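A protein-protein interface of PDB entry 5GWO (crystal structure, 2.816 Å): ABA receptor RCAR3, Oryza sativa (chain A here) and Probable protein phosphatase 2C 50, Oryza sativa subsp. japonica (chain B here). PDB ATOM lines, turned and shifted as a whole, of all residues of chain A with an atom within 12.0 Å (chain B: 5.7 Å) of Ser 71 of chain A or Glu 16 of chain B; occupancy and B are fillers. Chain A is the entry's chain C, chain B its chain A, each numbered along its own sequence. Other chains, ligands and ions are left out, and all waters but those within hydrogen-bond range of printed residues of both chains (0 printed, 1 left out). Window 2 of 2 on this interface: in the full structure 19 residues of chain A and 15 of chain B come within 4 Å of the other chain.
O of Pro 48 of chain A lies within hydrogen-bond range of ND2 of Asn 140 of chain B.
OE1 of Glu 16 of chain B lies within hydrogen-bond range of OG of Ser 71 of chain A (2.6 Å).
The backbone NH (N) of Gly 63 of chain B is in hydrogen-bond range of the side-chain hydroxyl (OG) of Ser 71 of chain A (2.8 Å).
The backbone NH (N) of Gly 64 of chain B lies within hydrogen-bond range of the side-chain carboxylate (OE2) of Glu 16 of chain B (3.4 Å).
The backbone carbonyl oxygen (O) of Pro 48 of chain A is in hydrogen-bond range of the side-chain amino group (NZ) of Lys 70 of chain A (2.7 Å).
The side-chain hydroxyl (OG) of Ser 51 of chain A sits at hydrogen-bond distance from the backbone NH (N) of Lys 70 of chain A, 2.8 Å away.
N of Glu 16 of chain B sits at hydrogen-bond distance from OD1 of Asn 311 of chain B.
The backbone carbonyl oxygen (O) of Glu 16 of chain B is in hydrogen-bond range of the backbone NH (N) of Gly 61 of chain B (2.8 Å).
O of Phe 49 of chain A is in hydrogen-bond range of N of Lys 70 of chain A (2.9 Å).
Phe 49 of chain A touches Asn 140 of chain B (CD1 to ND2, 3.5 Å).
Lys 70 of chain A touches Gly 63 of chain B.
Ser 71 of chain A touches His 62 of chain B (OG to CA, 3.2 Å).
Of the printed residues of chain B, Pro 48 of chain A touches Asn 140 (2.9 Å).
Of the printed residues of chain B, Phe 49 of chain A touches Asn 140.
Printed residues of chain B within 4 Å of Lys 70 of chain A: Gly 63.
Ser 71 of chain A touches just these residues of chain B: Glu 16, His 62 and Gly 63.
Glu 14 of chain B touches none of the printed residues of chain A.
Glu 16 of chain B touches one residue of chain A.
Ala 18 of chain B touches none of the printed residues of chain A.
No residue of chain A comes within 4 Å of Asp 60 of chain B.
No residue of chain A comes within 4 Å of Gly 61 of chain B.
His 62 of chain B touches just one residue of chain A: Ser 71.
Of chain A, only Lys 70 (3.6 Å) and Ser 71 (2.8 Å) come within 4 Å of Gly 63 of chain B.
No residue of chain A comes within 4 Å of Ala 65 of chain B.
No residue of chain A comes within 4 Å of Ala 68 of chain B.
Printed residues of chain A within 4 Å of Asn 140 of chain B: Pro 48 (2.9 Å) and Phe 49 (3.5 Å).
The nearest residue of chain B that does not touch Ser 71 of chain A is Gly 64 of chain B (4.3 Å).
The nearest residue of chain A that does not touch Glu 16 of chain B is Lys 70 of chain A (5.6 Å).
Printed residues of chain A that touch a printed residue of chain B: Pro 48, Phe 49, Lys 70 and Ser 71.
Of the 15 printed residues of chain B, 4 touch a printed residue of chain A.
Printed residues of chain B that touch a printed residue of chain A: Glu 16, His 62, Gly 63 and Asn 140.
Hydrophobic or aromatic side chains of chain B that line the printed part of chain A: His 62.
Among the printed residues, 6 pairs touch across the chains.
Among the printed residues, no Asp or Glu carboxylate lies within 4 Å of a Lys or Arg side-chain nitrogen of the other chain.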
ATOM      1  N   LYS A  47     -14.162  11.852  11.394  1.00  0.00           N
ATOM      2  CA  LYS A  47     -13.964  12.285  10.014  1.00  0.00           C
ATOM      3  C   LYS A  47     -13.163  11.266   9.218  1.00  0.00           C
ATOM      4  O   LYS A  47     -11.956  11.119   9.460  1.00  0.00           O
ATOM      5  CB  LYS A  47     -13.264  13.635   9.981  1.00  0.00           C
ATOM      6  CG  LYS A  47     -14.162  14.817  10.268  1.00  0.00           C
ATOM      7  CD  LYS A  47     -13.325  16.076  10.339  1.00  0.00           C
ATOM      8  CE  LYS A  47     -14.150  17.297  10.665  1.00  0.00           C
ATOM      9  NZ  LYS A  47     -15.103  17.603   9.579  1.00  0.00           N
ATOM     10  N   PRO A  48     -13.759  10.603   8.221  1.00  0.00           N
ATOM     11  CA  PRO A  48     -13.074   9.471   7.577  1.00  0.00           C
ATOM     12  C   PRO A  48     -11.966   9.858   6.623  1.00  0.00           C
ATOM     13  O   PRO A  48     -11.134   8.993   6.303  1.00  0.00           O
ATOM     14  CB  PRO A  48     -14.206   8.765   6.819  1.00  0.00           C
ATOM     15  CG  PRO A  48     -15.203   9.838   6.543  1.00  0.00           C
ATOM     16  CD  PRO A  48     -15.110  10.831   7.682  1.00  0.00           C
ATOM     17  N   PHE A  49     -11.919  11.107   6.156  1.00  0.00           N
ATOM     18  CA  PHE A  49     -10.899  11.532   5.205  1.00  0.00           C
ATOM     19  C   PHE A  49      -9.679  12.161   5.864  1.00  0.00           C
ATOM     20  O   PHE A  49      -8.796  12.650   5.158  1.00  0.00           O
ATOM     21  CB  PHE A  49     -11.495  12.491   4.187  1.00  0.00           C
ATOM     22  CG  PHE A  49     -12.406  11.834   3.189  1.00  0.00           C
ATOM     23  CD1 PHE A  49     -11.870  11.068   2.160  1.00  0.00           C
ATOM     24  CD2 PHE A  49     -13.784  12.025   3.234  1.00  0.00           C
ATOM     25  CE1 PHE A  49     -12.692  10.464   1.217  1.00  0.00           C
ATOM     26  CE2 PHE A  49     -14.622  11.423   2.289  1.00  0.00           C
ATOM     27  CZ  PHE A  49     -14.074  10.638   1.281  1.00  0.00           C
ATOM     28  N   VAL A  50      -9.589  12.128   7.190  1.00  0.00           N
ATOM     29  CA  VAL A  50      -8.486  12.737   7.924  1.00  0.00           C
ATOM     30  C   VAL A  50      -7.444  11.662   8.216  1.00  0.00           C
ATOM     31  O   VAL A  50      -7.735  10.668   8.897  1.00  0.00           O
ATOM     32  CB  VAL A  50      -8.972  13.392   9.224  1.00  0.00           C
ATOM     33  CG1 VAL A  50      -7.821  14.036   9.940  1.00  0.00           C
ATOM     34  CG2 VAL A  50     -10.068  14.406   8.937  1.00  0.00           C
ATOM     35  N   SER A  51      -6.220  11.887   7.732  1.00  0.00           N
ATOM     36  CA  SER A  51      -5.063  11.027   7.937  1.00  0.00           C
ATOM     37  C   SER A  51      -4.316  11.388   9.205  1.00  0.00           C
ATOM     38  O   SER A  51      -3.812  10.502   9.907  1.00  0.00           O
ATOM     39  CB  SER A  51      -4.081  11.168   6.772  1.00  0.00           C
ATOM     40  OG  SER A  51      -4.754  11.363   5.547  1.00  0.00           O
ATOM     41  N   ARG A  52      -4.226  12.685   9.488  1.00  0.00           N
ATOM     42  CA  ARG A  52      -3.506  13.196  10.639  1.00  0.00           C
ATOM     43  C   ARG A  52      -4.144  14.516  11.022  1.00  0.00           C
ATOM     44  O   ARG A  52      -4.977  15.056  10.292  1.00  0.00           O
ATOM     45  CB  ARG A  52      -2.008  13.346  10.334  1.00  0.00           C
ATOM     46  CG  ARG A  52      -1.345  12.012   9.992  1.00  0.00           C
ATOM     47  CD  ARG A  52       0.116  12.129   9.600  1.00  0.00           C
ATOM     48  NE  ARG A  52       0.274  12.924   8.387  1.00  0.00           N
ATOM     49  CZ  ARG A  52       1.442  13.199   7.817  1.00  0.00           C
ATOM     50  NH1 ARG A  52       2.568  12.732   8.342  1.00  0.00           N
ATOM     51  NH2 ARG A  52       1.480  13.935   6.713  1.00  0.00           N
ATOM     52  N   VAL A  67      -4.734  19.939   9.290  1.00  0.00           N
ATOM     53  CA  VAL A  67      -5.321  18.644   8.974  1.00  0.00           C
ATOM     54  C   VAL A  67      -4.739  18.138   7.664  1.00  0.00           C
ATOM     55  O   VAL A  67      -4.694  18.878   6.678  1.00  0.00           O
ATOM     56  CB  VAL A  67      -6.851  18.767   8.870  1.00  0.00           C
ATOM     57  CG1 VAL A  67      -7.453  17.515   8.306  1.00  0.00           C
ATOM     58  CG2 VAL A  67      -7.447  19.095  10.222  1.00  0.00           C
ATOM     59  N   ASN A  68      -4.341  16.873   7.635  1.00  0.00           N
ATOM     60  CA  ASN A  68      -3.952  16.204   6.401  1.00  0.00           C
ATOM     61  C   ASN A  68      -5.019  15.192   6.038  1.00  0.00           C
ATOM     62  O   ASN A  68      -5.487  14.454   6.905  1.00  0.00           O
ATOM     63  CB  ASN A  68      -2.612  15.478   6.536  1.00  0.00           C
ATOM     64  CG  ASN A  68      -1.456  16.415   6.590  1.00  0.00           C
ATOM     65  OD1 ASN A  68      -1.094  16.908   7.653  1.00  0.00           O
ATOM     66  ND2 ASN A  68      -0.872  16.688   5.438  1.00  0.00           N
ATOM     67  N   VAL A  69      -5.392  15.147   4.763  1.00  0.00           N
ATOM     68  CA  VAL A  69      -6.434  14.240   4.305  1.00  0.00           C
ATOM     69  C   VAL A  69      -5.813  13.104   3.502  1.00  0.00           C
ATOM     70  O   VAL A  69      -4.735  13.224   2.914  1.00  0.00           O
ATOM     71  CB  VAL A  69      -7.505  14.963   3.464  1.00  0.00           C
ATOM     72  CG1 VAL A  69      -8.367  15.855   4.351  1.00  0.00           C
ATOM     73  CG2 VAL A  69      -6.831  15.768   2.367  1.00  0.00           C
ATOM     74  N   LYS A  70      -6.541  11.994   3.450  1.00  0.00           N
ATOM     75  CA  LYS A  70      -6.080  10.818   2.736  1.00  0.00           C
ATOM     76  C   LYS A  70      -6.182  11.052   1.230  1.00  0.00           C
ATOM     77  O   LYS A  70      -6.784  12.021   0.756  1.00  0.00           O
ATOM     78  CB  LYS A  70      -6.910   9.598   3.135  1.00  0.00           C
ATOM     79  CG  LYS A  70      -7.042   9.393   4.631  1.00  0.00           C
ATOM     80  CD  LYS A  70      -7.795   8.114   4.926  1.00  0.00           C
ATOM     81  CE  LYS A  70      -7.805   7.791   6.416  1.00  0.00           C
ATOM     82  NZ  LYS A  70      -9.130   7.240   6.855  1.00  0.00           N
ATOM     83  N   SER A  71      -5.598  10.132   0.474  1.00  0.00           N
ATOM     84  CA  SER A  71      -5.614  10.220  -0.974  1.00  0.00           C
ATOM     85  C   SER A  71      -7.017   9.946  -1.500  1.00  0.00           C
ATOM     86  O   SER A  71      -7.921   9.551  -0.763  1.00  0.00           O
ATOM     87  CB  SER A  71      -4.602   9.248  -1.575  1.00  0.00           C
ATOM     88  OG  SER A  71      -4.686   7.987  -0.928  1.00  0.00           O
ATOM     89  N   GLY A  72      -7.203  10.210  -2.786  1.00  0.00           N
ATOM     90  CA  GLY A  72      -8.505  10.074  -3.406  1.00  0.00           C
ATOM     91  C   GLY A  72      -9.364  11.312  -3.328  1.00  0.00           C
ATOM     92  O   GLY A  72     -10.593  11.211  -3.433  1.00  0.00           O
ATOM     93  N   LEU A  73      -8.761  12.476  -3.159  1.00  0.00           N
ATOM     94  CA  LEU A  73      -9.491  13.724  -3.013  1.00  0.00           C
ATOM     95  C   LEU A  73      -8.754  14.802  -3.785  1.00  0.00           C
ATOM     96  O   LEU A  73      -7.574  14.646  -4.116  1.00  0.00           O
ATOM     97  CB  LEU A  73      -9.644  14.116  -1.534  1.00  0.00           C
ATOM     98  CG  LEU A  73     -10.569  13.281  -0.632  1.00  0.00           C
ATOM     99  CD1 LEU A  73     -10.354  13.638   0.829  1.00  0.00           C
ATOM    100  CD2 LEU A  73     -12.062  13.434  -0.997  1.00  0.00           C
ATOM    101  N   PRO A  74      -9.421  15.920  -4.084  1.00  0.00           N
ATOM    102  CA  PRO A  74      -8.792  16.978  -4.872  1.00  0.00           C
ATOM    103  C   PRO A  74      -7.834  17.865  -4.088  1.00  0.00           C
ATOM    104  O   PRO A  74      -7.241  18.774  -4.684  1.00  0.00           O
ATOM    105  CB  PRO A  74     -10.002  17.783  -5.377  1.00  0.00           C
ATOM    106  CG  PRO A  74     -11.221  17.271  -4.593  1.00  0.00           C
ATOM    107  CD  PRO A  74     -10.729  16.341  -3.556  1.00  0.00           C
ATOM    108  N   ALA A  75      -7.688  17.650  -2.776  1.00  0.00           N
ATOM    109  CA  ALA A  75      -6.770  18.411  -1.937  1.00  0.00           C
ATOM    110  C   ALA A  75      -6.097  17.464  -0.951  1.00  0.00           C
ATOM    111  O   ALA A  75      -6.541  16.333  -0.743  1.00  0.00           O
ATOM    112  CB  ALA A  75      -7.485  19.542  -1.185  1.00  0.00           C
ATOM    113  N   THR A  76      -5.055  17.961  -0.281  1.00  0.00           N
ATOM    114  CA  THR A  76      -4.275  17.146   0.641  1.00  0.00           C
ATOM    115  C   THR A  76      -4.151  17.715   2.050  1.00  0.00           C
ATOM    116  O   THR A  76      -3.794  16.957   2.962  1.00  0.00           O
ATOM    117  CB  THR A  76      -2.861  16.903   0.090  1.00  0.00           C
ATOM    118  OG1 THR A  76      -2.054  18.071   0.281  1.00  0.00           O
ATOM    119  CG2 THR A  76      -2.916  16.571  -1.392  1.00  0.00           C
ATOM    120  N   ARG A  77      -4.417  19.001   2.266  1.00  0.00           N
ATOM    121  CA  ARG A  77      -4.270  19.602   3.587  1.00  0.00           C
ATOM    122  C   ARG A  77      -5.261  20.744   3.741  1.00  0.00           C
ATOM    123  O   ARG A  77      -5.668  21.358   2.754  1.00  0.00           O
ATOM    124  CB  ARG A  77      -2.836  20.100   3.810  1.00  0.00           C
ATOM    125  CG  ARG A  77      -2.352  21.072   2.738  1.00  0.00           C
ATOM    126  CD  ARG A  77      -1.059  21.766   3.137  1.00  0.00           C
ATOM    127  NE  ARG A  77      -0.591  22.675   2.089  1.00  0.00           N
ATOM    128  CZ  ARG A  77      -0.928  23.961   1.993  1.00  0.00           C
ATOM    129  NH1 ARG A  77      -1.739  24.517   2.883  1.00  0.00           N
ATOM    130  NH2 ARG A  77      -0.448  24.690   0.999  1.00  0.00           N
ATOM    131  N   SER A  78      -5.656  21.016   4.986  1.00  0.00           N
ATOM    132  CA  SER A  78      -6.496  22.172   5.269  1.00  0.00           C
ATOM    133  C   SER A  78      -6.138  22.714   6.646  1.00  0.00           C
ATOM    134  O   SER A  78      -5.717  21.966   7.531  1.00  0.00           O
ATOM    135  CB  SER A  78      -7.992  21.839   5.195  1.00  0.00           C
ATOM    136  OG  SER A  78      -8.542  21.582   6.472  1.00  0.00           O
ATOM    137  N   ASP A 100      -4.564  23.744   0.793  1.00  0.00           N
ATOM    138  CA  ASP A 100      -4.299  23.710  -0.639  1.00  0.00           C
ATOM    139  C   ASP A 100      -5.546  23.345  -1.436  1.00  0.00           C
ATOM    140  O   ASP A 100      -5.445  22.819  -2.547  1.00  0.00           O
ATOM    141  CB  ASP A 100      -3.171  22.730  -0.948  1.00  0.00           C
ATOM    142  CG  ASP A 100      -3.579  21.279  -0.729  1.00  0.00           C
ATOM    143  OD1 ASP A 100      -4.642  21.029  -0.110  1.00  0.00           O
ATOM    144  OD2 ASP A 100      -2.816  20.383  -1.159  1.00  0.00           O
ATOM    145  N   PHE A 145     -20.432  19.004  -4.026  1.00  0.00           N
ATOM    146  CA  PHE A 145     -19.150  18.604  -3.458  1.00  0.00           C
ATOM    147  C   PHE A 145     -19.193  18.639  -1.931  1.00  0.00           C
ATOM    148  O   PHE A 145     -18.975  17.620  -1.256  1.00  0.00           O
ATOM    149  CB  PHE A 145     -18.049  19.518  -4.007  1.00  0.00           C
ATOM    150  CG  PHE A 145     -16.664  19.155  -3.551  1.00  0.00           C
ATOM    151  CD1 PHE A 145     -16.152  17.891  -3.777  1.00  0.00           C
ATOM    152  CD2 PHE A 145     -15.872  20.076  -2.900  1.00  0.00           C
ATOM    153  CE1 PHE A 145     -14.872  17.558  -3.362  1.00  0.00           C
ATOM    154  CE2 PHE A 145     -14.593  19.742  -2.479  1.00  0.00           C
ATOM    155  CZ  PHE A 145     -14.092  18.489  -2.713  1.00  0.00           C
ATOM    156  N   LEU A 149     -19.095  15.458   0.816  1.00  0.00           N
ATOM    157  CA  LEU A 149     -18.116  15.341   1.895  1.00  0.00           C
ATOM    158  C   LEU A 149     -18.780  15.305   3.271  1.00  0.00           C
ATOM    159  O   LEU A 149     -18.473  14.436   4.098  1.00  0.00           O
ATOM    160  CB  LEU A 149     -17.119  16.488   1.823  1.00  0.00           C
ATOM    161  CG  LEU A 149     -16.143  16.313   0.674  1.00  0.00           C
ATOM    162  CD1 LEU A 149     -15.131  17.464   0.676  1.00  0.00           C
ATOM    163  CD2 LEU A 149     -15.472  14.946   0.785  1.00  0.00           C
ATOM    164  N   CYS A 152     -20.529  12.024   4.071  1.00  0.00           N
ATOM    165  CA  CYS A 152     -19.554  11.044   4.546  1.00  0.00           C
ATOM    166  C   CYS A 152     -19.209  11.278   6.006  1.00  0.00           C
ATOM    167  O   CYS A 152     -19.223  10.345   6.822  1.00  0.00           O
ATOM    168  CB  CYS A 152     -18.291  11.105   3.702  1.00  0.00           C
ATOM    169  SG  CYS A 152     -18.522  10.401   2.113  1.00  0.00           S
ATOM    170  N   ASN A 153     -18.895  12.529   6.352  1.00  0.00           N
ATOM    171  CA  ASN A 153     -18.498  12.843   7.719  1.00  0.00           C
ATOM    172  C   ASN A 153     -19.564  12.441   8.718  1.00  0.00           C
ATOM    173  O   ASN A 153     -19.259  11.844   9.753  1.00  0.00           O
ATOM    174  CB  ASN A 153     -18.191  14.325   7.841  1.00  0.00           C
ATOM    175  CG  ASN A 153     -16.890  14.666   7.222  1.00  0.00           C
ATOM    176  OD1 ASN A 153     -16.096  13.778   6.902  1.00  0.00           O
ATOM    177  ND2 ASN A 153     -16.632  15.951   7.066  1.00  0.00           N
ATOM    178  N   GLU B  14       3.258   7.992   2.669  1.00  0.00           N
ATOM    179  CA  GLU B  14       2.957   6.577   2.812  1.00  0.00           C
ATOM    180  C   GLU B  14       2.953   5.899   1.449  1.00  0.00           C
ATOM    181  O   GLU B  14       2.761   6.533   0.408  1.00  0.00           O
ATOM    182  CB  GLU B  14       1.596   6.367   3.490  1.00  0.00           C
ATOM    183  CG  GLU B  14       1.418   7.097   4.808  1.00  0.00           C
ATOM    184  CD  GLU B  14      -0.028   7.091   5.284  1.00  0.00           C
ATOM    185  OE1 GLU B  14      -0.933   7.312   4.451  1.00  0.00           O
ATOM    186  OE2 GLU B  14      -0.262   6.874   6.491  1.00  0.00           O
ATOM    187  N   MET B  15       3.164   4.590   1.469  1.00  0.00           N
ATOM    188  CA  MET B  15       3.101   3.769   0.268  1.00  0.00           C
ATOM    189  C   MET B  15       1.717   3.140   0.184  1.00  0.00           C
ATOM    190  O   MET B  15       1.301   2.423   1.099  1.00  0.00           O
ATOM    191  CB  MET B  15       4.174   2.683   0.269  1.00  0.00           C
ATOM    192  CG  MET B  15       4.126   1.789  -0.958  1.00  0.00           C
ATOM    193  SD  MET B  15       4.133   2.741  -2.498  1.00  0.00           S
ATOM    194  CE  MET B  15       4.967   1.609  -3.603  1.00  0.00           C
ATOM    195  N   GLU B  16       0.981   3.468  -0.872  1.00  0.00           N
ATOM    196  CA  GLU B  16      -0.340   2.899  -1.093  1.00  0.00           C
ATOM    197  C   GLU B  16      -0.442   2.197  -2.444  1.00  0.00           C
ATOM    198  O   GLU B  16      -1.544   1.841  -2.874  1.00  0.00           O
ATOM    199  CB  GLU B  16      -1.408   3.983  -0.932  1.00  0.00           C
ATOM    200  CG  GLU B  16      -1.470   4.529   0.490  1.00  0.00           C
ATOM    201  CD  GLU B  16      -2.494   5.632   0.660  1.00  0.00           C
ATOM    202  OE1 GLU B  16      -3.049   6.090  -0.363  1.00  0.00           O
ATOM    203  OE2 GLU B  16      -2.740   6.046   1.818  1.00  0.00           O
ATOM    204  N   ASP B  17       0.665   2.022  -3.142  1.00  0.00           N
ATOM    205  CA  ASP B  17       0.660   1.205  -4.341  1.00  0.00           C
ATOM    206  C   ASP B  17       1.051  -0.226  -3.983  1.00  0.00           C
ATOM    207  O   ASP B  17       1.675  -0.491  -2.950  1.00  0.00           O
ATOM    208  CB  ASP B  17       1.604   1.781  -5.402  1.00  0.00           C
ATOM    209  CG  ASP B  17       0.998   2.974  -6.149  1.00  0.00           C
ATOM    210  OD1 ASP B  17       0.103   3.649  -5.587  1.00  0.00           O
ATOM    211  OD2 ASP B  17       1.428   3.250  -7.294  1.00  0.00           O
ATOM    212  N   ALA B  18       0.623  -1.159  -4.829  1.00  0.00           N
ATOM    213  CA  ALA B  18       0.991  -2.557  -4.685  1.00  0.00           C
ATOM    214  C   ALA B  18       1.092  -3.156  -6.076  1.00  0.00           C
ATOM    215  O   ALA B  18       0.626  -2.575  -7.058  1.00  0.00           O
ATOM    216  CB  ALA B  18      -0.016  -3.334  -3.830  1.00  0.00           C
ATOM    217  N   PHE B  59      -1.695  -2.071  -8.670  1.00  0.00           N
ATOM    218  CA  PHE B  59      -2.838  -1.663  -7.861  1.00  0.00           C
ATOM    219  C   PHE B  59      -2.477  -0.350  -7.176  1.00  0.00           C
ATOM    220  O   PHE B  59      -1.762  -0.331  -6.170  1.00  0.00           O
ATOM    221  CB  PHE B  59      -3.230  -2.756  -6.859  1.00  0.00           C
ATOM    222  CG  PHE B  59      -3.206  -4.145  -7.443  1.00  0.00           C
ATOM    223  CD1 PHE B  59      -4.243  -4.593  -8.243  1.00  0.00           C
ATOM    224  CD2 PHE B  59      -2.150  -5.005  -7.187  1.00  0.00           C
ATOM    225  CE1 PHE B  59      -4.217  -5.866  -8.797  1.00  0.00           C
ATOM    226  CE2 PHE B  59      -2.128  -6.282  -7.729  1.00  0.00           C
ATOM    227  CZ  PHE B  59      -3.162  -6.708  -8.534  1.00  0.00           C
ATOM    228  N   ASP B  60      -2.955   0.753  -7.743  1.00  0.00           N
ATOM    229  CA  ASP B  60      -2.765   2.068  -7.147  1.00  0.00           C
ATOM    230  C   ASP B  60      -3.863   2.259  -6.112  1.00  0.00           C
ATOM    231  O   ASP B  60      -5.036   2.446  -6.460  1.00  0.00           O
ATOM    232  CB  ASP B  60      -2.790   3.159  -8.215  1.00  0.00           C
ATOM    233  CG  ASP B  60      -2.618   4.557  -7.636  1.00  0.00           C
ATOM    234  OD1 ASP B  60      -2.466   4.691  -6.398  1.00  0.00           O
ATOM    235  OD2 ASP B  60      -2.613   5.524  -8.436  1.00  0.00           O
ATOM    236  N   GLY B  61      -3.493   2.166  -4.841  1.00  0.00           N
ATOM    237  CA  GLY B  61      -4.454   2.392  -3.796  1.00  0.00           C
ATOM    238  C   GLY B  61      -4.676   3.866  -3.532  1.00  0.00           C
ATOM    239  O   GLY B  61      -3.892   4.736  -3.928  1.00  0.00           O
ATOM    240  N   HIS B  62      -5.794   4.144  -2.869  1.00  0.00           N
ATOM    241  CA  HIS B  62      -6.113   5.489  -2.437  1.00  0.00           C
ATOM    242  C   HIS B  62      -6.993   5.408  -1.198  1.00  0.00           C
ATOM    243  O   HIS B  62      -7.707   4.422  -0.987  1.00  0.00           O
ATOM    244  CB  HIS B  62      -6.767   6.280  -3.564  1.00  0.00           C
ATOM    245  CG  HIS B  62      -7.985   5.633  -4.125  1.00  0.00           C
ATOM    246  ND1 HIS B  62      -8.075   5.241  -5.440  1.00  0.00           N
ATOM    247  CD2 HIS B  62      -9.160   5.287  -3.545  1.00  0.00           C
ATOM    248  CE1 HIS B  62      -9.254   4.688  -5.650  1.00  0.00           C
ATOM    249  NE2 HIS B  62      -9.931   4.699  -4.517  1.00  0.00           N
ATOM    250  N   GLY B  63      -6.907   6.441  -0.363  1.00  0.00           N
ATOM    251  CA  GLY B  63      -7.603   6.419   0.906  1.00  0.00           C
ATOM    252  C   GLY B  63      -7.088   5.383   1.871  1.00  0.00           C
ATOM    253  O   GLY B  63      -7.731   5.141   2.900  1.00  0.00           O
ATOM    254  N   GLY B  64      -5.935   4.794   1.585  1.00  0.00           N
ATOM    255  CA  GLY B  64      -5.409   3.654   2.311  1.00  0.00           C
ATOM    256  C   GLY B  64      -4.817   2.647   1.342  1.00  0.00           C
ATOM    257  O   GLY B  64      -5.077   2.670   0.140  1.00  0.00           O
ATOM    258  N   ALA B  65      -3.951   1.779   1.869  1.00  0.00           N
ATOM    259  CA  ALA B  65      -3.318   0.720   1.084  1.00  0.00           C
ATOM    260  C   ALA B  65      -4.006  -0.632   1.213  1.00  0.00           C
ATOM    261  O   ALA B  65      -3.601  -1.580   0.534  1.00  0.00           O
ATOM    262  CB  ALA B  65      -1.849   0.563   1.489  1.00  0.00           C
ATOM    263  N   ALA B  68      -5.484  -2.133  -2.217  1.00  0.00           N
ATOM    264  CA  ALA B  68      -4.470  -2.543  -3.184  1.00  0.00           C
ATOM    265  C   ALA B  68      -3.750  -3.805  -2.719  1.00  0.00           C
ATOM    266  O   ALA B  68      -3.473  -4.704  -3.525  1.00  0.00           O
ATOM    267  CB  ALA B  68      -3.477  -1.407  -3.430  1.00  0.00           C
ATOM    268  N   ASN B 140     -14.148   4.605   2.174  1.00  0.00           N
ATOM    269  CA  ASN B 140     -13.456   5.569   1.330  1.00  0.00           C
ATOM    270  C   ASN B 140     -12.131   5.034   0.812  1.00  0.00           C
ATOM    271  O   ASN B 140     -11.400   5.766   0.136  1.00  0.00           O
ATOM    272  CB  ASN B 140     -13.245   6.882   2.089  1.00  0.00           C
ATOM    273  CG  ASN B 140     -12.248   6.748   3.226  1.00  0.00           C
ATOM    274  OD1 ASN B 140     -11.940   5.641   3.683  1.00  0.00           O
ATOM    275  ND2 ASN B 140     -11.761   7.884   3.715  1.00  0.00           N
ATOM    276  N   ASN B 311       3.056   7.759  -5.439  1.00  0.00           N
ATOM    277  CA  ASN B 311       3.676   6.444  -5.397  1.00  0.00           C
ATOM    278  C   ASN B 311       3.900   5.969  -6.826  1.00  0.00           C
ATOM    279  O   ASN B 311       3.037   6.142  -7.693  1.00  0.00           O
ATOM    280  CB  ASN B 311       2.793   5.434  -4.660  1.00  0.00           C
ATOM    281  CG  ASN B 311       2.377   5.894  -3.276  1.00  0.00           C
ATOM    282  OD1 ASN B 311       1.322   5.484  -2.773  1.00  0.00           O
ATOM    283  ND2 ASN B 311       3.201   6.732  -2.644  1.00  0.00           N
